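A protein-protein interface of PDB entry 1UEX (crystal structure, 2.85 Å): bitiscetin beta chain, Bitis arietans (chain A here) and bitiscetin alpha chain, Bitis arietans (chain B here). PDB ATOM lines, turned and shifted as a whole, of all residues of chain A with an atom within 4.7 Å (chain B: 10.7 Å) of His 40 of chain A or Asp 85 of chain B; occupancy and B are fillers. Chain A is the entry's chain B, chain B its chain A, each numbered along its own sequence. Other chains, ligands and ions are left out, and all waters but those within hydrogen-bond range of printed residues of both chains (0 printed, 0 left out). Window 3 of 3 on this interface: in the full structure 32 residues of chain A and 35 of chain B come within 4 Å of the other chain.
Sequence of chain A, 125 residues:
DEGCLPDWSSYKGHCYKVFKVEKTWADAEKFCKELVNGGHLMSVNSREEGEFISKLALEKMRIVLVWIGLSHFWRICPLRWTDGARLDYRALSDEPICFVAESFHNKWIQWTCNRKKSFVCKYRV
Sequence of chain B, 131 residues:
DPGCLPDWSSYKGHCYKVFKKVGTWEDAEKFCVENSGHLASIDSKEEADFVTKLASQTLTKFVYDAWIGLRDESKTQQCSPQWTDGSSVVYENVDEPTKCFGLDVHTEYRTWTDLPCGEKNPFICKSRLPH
ND1 of His 40 of chain A sits close to O of Thr 84 of chain B (3.4 Å).
The side-chain hydroxyl (OG) of Ser 43 of chain A lies within hydrogen-bond range of the side-chain carboxylate (OD1) of Asp 85 of chain B.
The side-chain hydroxyl (OG1) of Thr 84 of chain B sits close to the side-chain carboxylate (OE2) of Glu 29 of chain A (3.3 Å).
The side-chain carboxylate (OE2) of Glu 29 of chain A is in hydrogen-bond range of a ring nitrogen (ND1) of His 40 of chain A (2.7 Å).
The side-chain sulfur of Cys 121 of chain A forms a disulfide with the side-chain sulfur of Cys 32 of chain A (2.0 Å).
N of Met 42 of chain A sits close to O of Val 120 of chain A (3.4 Å).
The side-chain carboxylate (OE1) of Glu 29 of chain A is in hydrogen-bond range of the backbone NH (N) of Leu 41 of chain A (2.6 Å).
The backbone NH of Ser 87 of chain B sits at hydrogen-bond distance from the side-chain carboxylate of Asp 85 of chain B (2.7 Å).
The backbone carbonyl oxygen of His 40 of chain A sits at hydrogen-bond distance from the backbone NH of Lys 122 of chain A.
Among the printed residues, pairs that only touch across the chains: His 40 of chain A with Asp 85 of chain B, Leu 41 of chain A with Thr 84 of chain B, Met 42 of chain A with Trp 83 of chain B, Ser 43 of chain A with Trp 83 of chain B and Ser 43 of chain A with Ser 87 of chain B.
Of chain B, only Thr 84 (3.3 Å) and Asp 85 (3.4 Å) come within 4 Å of His 40 of chain A.
Of chain A, only His 40 (3.4 Å) and Ser 43 (2.6 Å) come within 4 Å of Asp 85 of chain B.
No residue of chain B comes within 4 Å of Gly 39 of chain A.
No residue of chain B comes within 4 Å of Cys 121 of chain A.
No residue of chain B comes within 4 Å of Lys 122 of chain A.
Printed residues of chain A within 4 Å of Trp 83 of chain B: Met 42 (3.9 Å) and Ser 43 (3.4 Å).
Of the printed residues of chain A, Thr 84 of chain B touches Glu 29, His 40 and Leu 41.
Printed residues of chain A within 4 Å of Ser 87 of chain B: Ser 43.
Printed residues of chain B within 4 Å of Met 42 of chain A: Trp 83.
Gly 86 of chain B touches none of the printed residues of chain A.
Pro 81 of chain B touches none of the printed residues of chain A.
The nearest residue of chain B that does not touch His 40 of chain A is Gly 86 of chain B (5.5 Å).
The nearest printed residue of chain A that does not touch Thr 84 of chain B is Met 42 of chain A (5.3 Å).
Hydrophobic or aromatic side chains of chain B within 4 Å of the printed part of chain A: Trp 83.
Of the 12 printed residues of chain A, 5 touch a printed residue of chain B.
Hydrophobic or aromatic side chains of chain A that line the printed part of chain B: His 40.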
ATOM      1  N   GLU A  29     -16.641 -26.059  13.963  1.00  0.00           N
ATOM      2  CA  GLU A  29     -17.854 -25.261  14.049  1.00  0.00           C
ATOM      3  C   GLU A  29     -18.489 -25.204  12.670  1.00  0.00           C
ATOM      4  O   GLU A  29     -19.693 -25.411  12.519  1.00  0.00           O
ATOM      5  CB  GLU A  29     -17.531 -23.843  14.532  1.00  0.00           C
ATOM      6  CG  GLU A  29     -18.655 -22.825  14.307  1.00  0.00           C
ATOM      7  CD  GLU A  29     -19.915 -23.113  15.115  1.00  0.00           C
ATOM      8  OE1 GLU A  29     -20.069 -24.242  15.623  1.00  0.00           O
ATOM      9  OE2 GLU A  29     -20.764 -22.202  15.230  1.00  0.00           O
ATOM     10  N   CYS A  32     -20.202 -28.338  12.003  1.00  0.00           N
ATOM     11  CA  CYS A  32     -21.473 -28.544  12.693  1.00  0.00           C
ATOM     12  C   CYS A  32     -22.587 -27.785  11.987  1.00  0.00           C
ATOM     13  O   CYS A  32     -23.743 -28.205  12.004  1.00  0.00           O
ATOM     14  CB  CYS A  32     -21.401 -28.052  14.138  1.00  0.00           C
ATOM     15  SG  CYS A  32     -20.289 -28.949  15.266  1.00  0.00           S
ATOM     16  N   LYS A  33     -22.234 -26.660  11.376  1.00  0.00           N
ATOM     17  CA  LYS A  33     -23.215 -25.842  10.683  1.00  0.00           C
ATOM     18  C   LYS A  33     -23.652 -26.439   9.355  1.00  0.00           C
ATOM     19  O   LYS A  33     -24.846 -26.643   9.122  1.00  0.00           O
ATOM     20  CB  LYS A  33     -22.675 -24.425  10.461  1.00  0.00           C
ATOM     21  CG  LYS A  33     -22.593 -23.590  11.730  1.00  0.00           C
ATOM     22  CD  LYS A  33     -22.389 -22.116  11.425  1.00  0.00           C
ATOM     23  CE  LYS A  33     -21.058 -21.857  10.751  1.00  0.00           C
ATOM     24  NZ  LYS A  33     -20.881 -20.414  10.440  1.00  0.00           N
ATOM     25  N   GLY A  38     -29.037 -25.108  11.667  1.00  0.00           N
ATOM     26  CA  GLY A  38     -29.037 -24.524  12.995  1.00  0.00           C
ATOM     27  C   GLY A  38     -28.214 -25.339  13.974  1.00  0.00           C
ATOM     28  O   GLY A  38     -28.498 -25.373  15.170  1.00  0.00           O
ATOM     29  N   GLY A  39     -27.197 -26.014  13.460  1.00  0.00           N
ATOM     30  CA  GLY A  39     -26.346 -26.809  14.317  1.00  0.00           C
ATOM     31  C   GLY A  39     -25.128 -25.980  14.645  1.00  0.00           C
ATOM     32  O   GLY A  39     -24.766 -25.081  13.882  1.00  0.00           O
ATOM     33  N   HIS A  40     -24.499 -26.270  15.779  1.00  0.00           N
ATOM     34  CA  HIS A  40     -23.317 -25.535  16.201  1.00  0.00           C
ATOM     35  C   HIS A  40     -22.369 -26.390  17.036  1.00  0.00           C
ATOM     36  O   HIS A  40     -22.667 -27.535  17.367  1.00  0.00           O
ATOM     37  CB  HIS A  40     -23.729 -24.282  16.981  1.00  0.00           C
ATOM     38  CG  HIS A  40     -24.284 -23.187  16.119  1.00  0.00           C
ATOM     39  ND1 HIS A  40     -23.497 -22.422  15.288  1.00  0.00           N
ATOM     40  CD2 HIS A  40     -25.555 -22.746  15.953  1.00  0.00           C
ATOM     41  CE1 HIS A  40     -24.258 -21.552  14.643  1.00  0.00           C
ATOM     42  NE2 HIS A  40     -25.507 -21.729  15.030  1.00  0.00           N
ATOM     43  N   LEU A  41     -21.237 -25.800  17.395  1.00  0.00           N
ATOM     44  CA  LEU A  41     -20.188 -26.480  18.146  1.00  0.00           C
ATOM     45  C   LEU A  41     -20.386 -26.761  19.638  1.00  0.00           C
ATOM     46  O   LEU A  41     -19.422 -26.722  20.392  1.00  0.00           O
ATOM     47  CB  LEU A  41     -18.880 -25.708  17.959  1.00  0.00           C
ATOM     48  CG  LEU A  41     -17.557 -26.392  18.296  1.00  0.00           C
ATOM     49  CD1 LEU A  41     -17.362 -27.625  17.436  1.00  0.00           C
ATOM     50  CD2 LEU A  41     -16.444 -25.410  18.057  1.00  0.00           C
ATOM     51  N   MET A  42     -21.608 -27.055  20.072  1.00  0.00           N
ATOM     52  CA  MET A  42     -21.847 -27.360  21.487  1.00  0.00           C
ATOM     53  C   MET A  42     -21.608 -26.180  22.434  1.00  0.00           C
ATOM     54  O   MET A  42     -20.512 -25.621  22.487  1.00  0.00           O
ATOM     55  CB  MET A  42     -20.951 -28.524  21.927  1.00  0.00           C
ATOM     56  CG  MET A  42     -21.077 -28.891  23.403  1.00  0.00           C
ATOM     57  SD  MET A  42     -19.737 -29.958  24.030  1.00  0.00           S
ATOM     58  CE  MET A  42     -19.173 -29.031  25.438  1.00  0.00           C
ATOM     59  N   SER A  43     -22.639 -25.810  23.186  1.00  0.00           N
ATOM     60  CA  SER A  43     -22.543 -24.720  24.153  1.00  0.00           C
ATOM     61  C   SER A  43     -23.114 -25.231  25.466  1.00  0.00           C
ATOM     62  O   SER A  43     -24.162 -25.873  25.477  1.00  0.00           O
ATOM     63  CB  SER A  43     -23.331 -23.493  23.675  1.00  0.00           C
ATOM     64  OG  SER A  43     -24.687 -23.805  23.418  1.00  0.00           O
ATOM     65  N   VAL A 120     -17.803 -31.731  19.565  1.00  0.00           N
ATOM     66  CA  VAL A 120     -19.195 -32.065  19.815  1.00  0.00           C
ATOM     67  C   VAL A 120     -20.060 -31.027  19.122  1.00  0.00           C
ATOM     68  O   VAL A 120     -19.813 -29.829  19.251  1.00  0.00           O
ATOM     69  CB  VAL A 120     -19.520 -32.048  21.337  1.00  0.00           C
ATOM     70  CG1 VAL A 120     -21.013 -32.259  21.560  1.00  0.00           C
ATOM     71  CG2 VAL A 120     -18.719 -33.124  22.059  1.00  0.00           C
ATOM     72  N   CYS A 121     -21.056 -31.489  18.372  1.00  0.00           N
ATOM     73  CA  CYS A 121     -21.972 -30.592  17.680  1.00  0.00           C
ATOM     74  C   CYS A 121     -23.284 -30.529  18.458  1.00  0.00           C
ATOM     75  O   CYS A 121     -23.589 -31.429  19.243  1.00  0.00           O
ATOM     76  CB  CYS A 121     -22.234 -31.074  16.256  1.00  0.00           C
ATOM     77  SG  CYS A 121     -20.848 -30.890  15.089  1.00  0.00           S
ATOM     78  N   LYS A 122     -24.067 -29.478  18.225  1.00  0.00           N
ATOM     79  CA  LYS A 122     -25.325 -29.291  18.946  1.00  0.00           C
ATOM     80  C   LYS A 122     -26.363 -28.478  18.173  1.00  0.00           C
ATOM     81  O   LYS A 122     -26.058 -27.420  17.629  1.00  0.00           O
ATOM     82  CB  LYS A 122     -25.010 -28.609  20.280  1.00  0.00           C
ATOM     83  CG  LYS A 122     -26.178 -28.027  21.056  1.00  0.00           C
ATOM     84  CD  LYS A 122     -25.627 -27.141  22.183  1.00  0.00           C
ATOM     85  CE  LYS A 122     -26.709 -26.393  22.950  1.00  0.00           C
ATOM     86  NZ  LYS A 122     -27.486 -27.286  23.847  1.00  0.00           N
ATOM     87  N   SER B  80     -15.538 -14.142  26.475  1.00  0.00           N
ATOM     88  CA  SER B  80     -16.478 -14.251  25.364  1.00  0.00           C
ATOM     89  C   SER B  80     -17.902 -14.124  25.904  1.00  0.00           C
ATOM     90  O   SER B  80     -18.341 -14.938  26.715  1.00  0.00           O
ATOM     91  CB  SER B  80     -16.304 -15.591  24.648  1.00  0.00           C
ATOM     92  OG  SER B  80     -17.221 -15.731  23.578  1.00  0.00           O
ATOM     93  N   PRO B  81     -18.641 -13.093  25.463  1.00  0.00           N
ATOM     94  CA  PRO B  81     -20.017 -12.858  25.905  1.00  0.00           C
ATOM     95  C   PRO B  81     -21.080 -13.703  25.211  1.00  0.00           C
ATOM     96  O   PRO B  81     -22.134 -13.968  25.785  1.00  0.00           O
ATOM     97  CB  PRO B  81     -20.206 -11.377  25.633  1.00  0.00           C
ATOM     98  CG  PRO B  81     -19.458 -11.202  24.366  1.00  0.00           C
ATOM     99  CD  PRO B  81     -18.171 -11.968  24.634  1.00  0.00           C
ATOM    100  N   GLN B  82     -20.810 -14.122  23.981  1.00  0.00           N
ATOM    101  CA  GLN B  82     -21.771 -14.927  23.232  1.00  0.00           C
ATOM    102  C   GLN B  82     -21.144 -16.240  22.777  1.00  0.00           C
ATOM    103  O   GLN B  82     -19.924 -16.323  22.600  1.00  0.00           O
ATOM    104  CB  GLN B  82     -22.248 -14.157  21.995  1.00  0.00           C
ATOM    105  CG  GLN B  82     -23.758 -14.103  21.796  1.00  0.00           C
ATOM    106  CD  GLN B  82     -24.444 -13.125  22.745  1.00  0.00           C
ATOM    107  OE1 GLN B  82     -24.073 -11.950  22.816  1.00  0.00           O
ATOM    108  NE2 GLN B  82     -25.450 -13.606  23.471  1.00  0.00           N
ATOM    109  N   TRP B  83     -21.978 -17.265  22.600  1.00  0.00           N
ATOM    110  CA  TRP B  83     -21.496 -18.557  22.114  1.00  0.00           C
ATOM    111  C   TRP B  83     -21.587 -18.525  20.587  1.00  0.00           C
ATOM    112  O   TRP B  83     -22.036 -17.533  20.007  1.00  0.00           O
ATOM    113  CB  TRP B  83     -22.347 -19.715  22.646  1.00  0.00           C
ATOM    114  CG  TRP B  83     -22.139 -20.032  24.091  1.00  0.00           C
ATOM    115  CD1 TRP B  83     -22.762 -19.454  25.153  1.00  0.00           C
ATOM    116  CD2 TRP B  83     -21.244 -21.012  24.635  1.00  0.00           C
ATOM    117  NE1 TRP B  83     -22.312 -20.011  26.332  1.00  0.00           N
ATOM    118  CE2 TRP B  83     -21.374 -20.965  26.040  1.00  0.00           C
ATOM    119  CE3 TRP B  83     -20.332 -21.913  24.072  1.00  0.00           C
ATOM    120  CZ2 TRP B  83     -20.644 -21.799  26.891  1.00  0.00           C
ATOM    121  CZ3 TRP B  83     -19.602 -22.743  24.920  1.00  0.00           C
ATOM    122  CH2 TRP B  83     -19.758 -22.674  26.314  1.00  0.00           C
ATOM    123  N   THR B  84     -21.156 -19.599  19.936  1.00  0.00           N
ATOM    124  CA  THR B  84     -21.214 -19.652  18.481  1.00  0.00           C
ATOM    125  C   THR B  84     -22.648 -19.810  18.002  1.00  0.00           C
ATOM    126  O   THR B  84     -22.973 -19.432  16.880  1.00  0.00           O
ATOM    127  CB  THR B  84     -20.394 -20.821  17.917  1.00  0.00           C
ATOM    128  OG1 THR B  84     -20.794 -22.041  18.557  1.00  0.00           O
ATOM    129  CG2 THR B  84     -18.922 -20.587  18.145  1.00  0.00           C
ATOM    130  N   ASP B  85     -23.501 -20.368  18.858  1.00  0.00           N
ATOM    131  CA  ASP B  85     -24.907 -20.584  18.521  1.00  0.00           C
ATOM    132  C   ASP B  85     -25.786 -19.382  18.847  1.00  0.00           C
ATOM    133  O   ASP B  85     -27.004 -19.426  18.637  1.00  0.00           O
ATOM    134  CB  ASP B  85     -25.453 -21.807  19.259  1.00  0.00           C
ATOM    135  CG  ASP B  85     -25.429 -21.636  20.756  1.00  0.00           C
ATOM    136  OD1 ASP B  85     -25.934 -22.525  21.469  1.00  0.00           O
ATOM    137  OD2 ASP B  85     -24.900 -20.607  21.219  1.00  0.00           O
ATOM    138  N   GLY B  86     -25.168 -18.319  19.362  1.00  0.00           N
ATOM    139  CA  GLY B  86     -25.910 -17.123  19.710  1.00  0.00           C
ATOM    140  C   GLY B  86     -26.338 -17.120  21.165  1.00  0.00           C
ATOM    141  O   GLY B  86     -26.930 -16.150  21.637  1.00  0.00           O
ATOM    142  N   SER B  87     -26.053 -18.210  21.872  1.00  0.00           N
ATOM    143  CA  SER B  87     -26.400 -18.317  23.286  1.00  0.00           C
ATOM    144  C   SER B  87     -25.600 -17.312  24.110  1.00  0.00           C
ATOM    145  O   SER B  87     -24.421 -17.067  23.848  1.00  0.00           O
ATOM    146  CB  SER B  87     -26.111 -19.728  23.816  1.00  0.00           C
ATOM    147  OG  SER B  87     -27.021 -20.687  23.305  1.00  0.00           O
ATOM    148  N   SER B  88     -26.250 -16.722  25.102  1.00  0.00           N
ATOM    149  CA  SER B  88     -25.584 -15.765  25.963  1.00  0.00           C
ATOM    150  C   SER B  88     -24.774 -16.612  26.931  1.00  0.00           C
ATOM    151  O   SER B  88     -25.241 -17.662  27.384  1.00  0.00           O
ATOM    152  CB  SER B  88     -26.623 -14.926  26.721  1.00  0.00           C
ATOM    153  OG  SER B  88     -26.046 -13.763  27.300  1.00  0.00           O
ATOM    154  N   VAL B  89     -23.552 -16.182  27.227  1.00  0.00           N
ATOM    155  CA  VAL B  89     -22.715 -16.931  28.153  1.00  0.00           C
ATOM    156  C   VAL B  89     -23.144 -16.613  29.577  1.00  0.00           C
ATOM    157  O   VAL B  89     -22.721 -15.618  30.163  1.00  0.00           O
ATOM    158  CB  VAL B  89     -21.225 -16.586  27.993  1.00  0.00           C
ATOM    159  CG1 VAL B  89     -20.390 -17.514  28.867  1.00  0.00           C
ATOM    160  CG2 VAL B  89     -20.810 -16.716  26.536  1.00  0.00           C
ATOM    161  N   VAL B  90     -23.999 -17.466  30.118  1.00  0.00           N
ATOM    162  CA  VAL B  90     -24.507 -17.286  31.465  1.00  0.00           C
ATOM    163  C   VAL B  90     -23.687 -18.108  32.441  1.00  0.00           C
ATOM    164  O   VAL B  90     -23.018 -17.567  33.320  1.00  0.00           O
ATOM    165  CB  VAL B  90     -25.975 -17.729  31.549  1.00  0.00           C
ATOM    166  CG1 VAL B  90     -26.427 -17.777  33.000  1.00  0.00           C
ATOM    167  CG2 VAL B  90     -26.837 -16.780  30.746  1.00  0.00           C
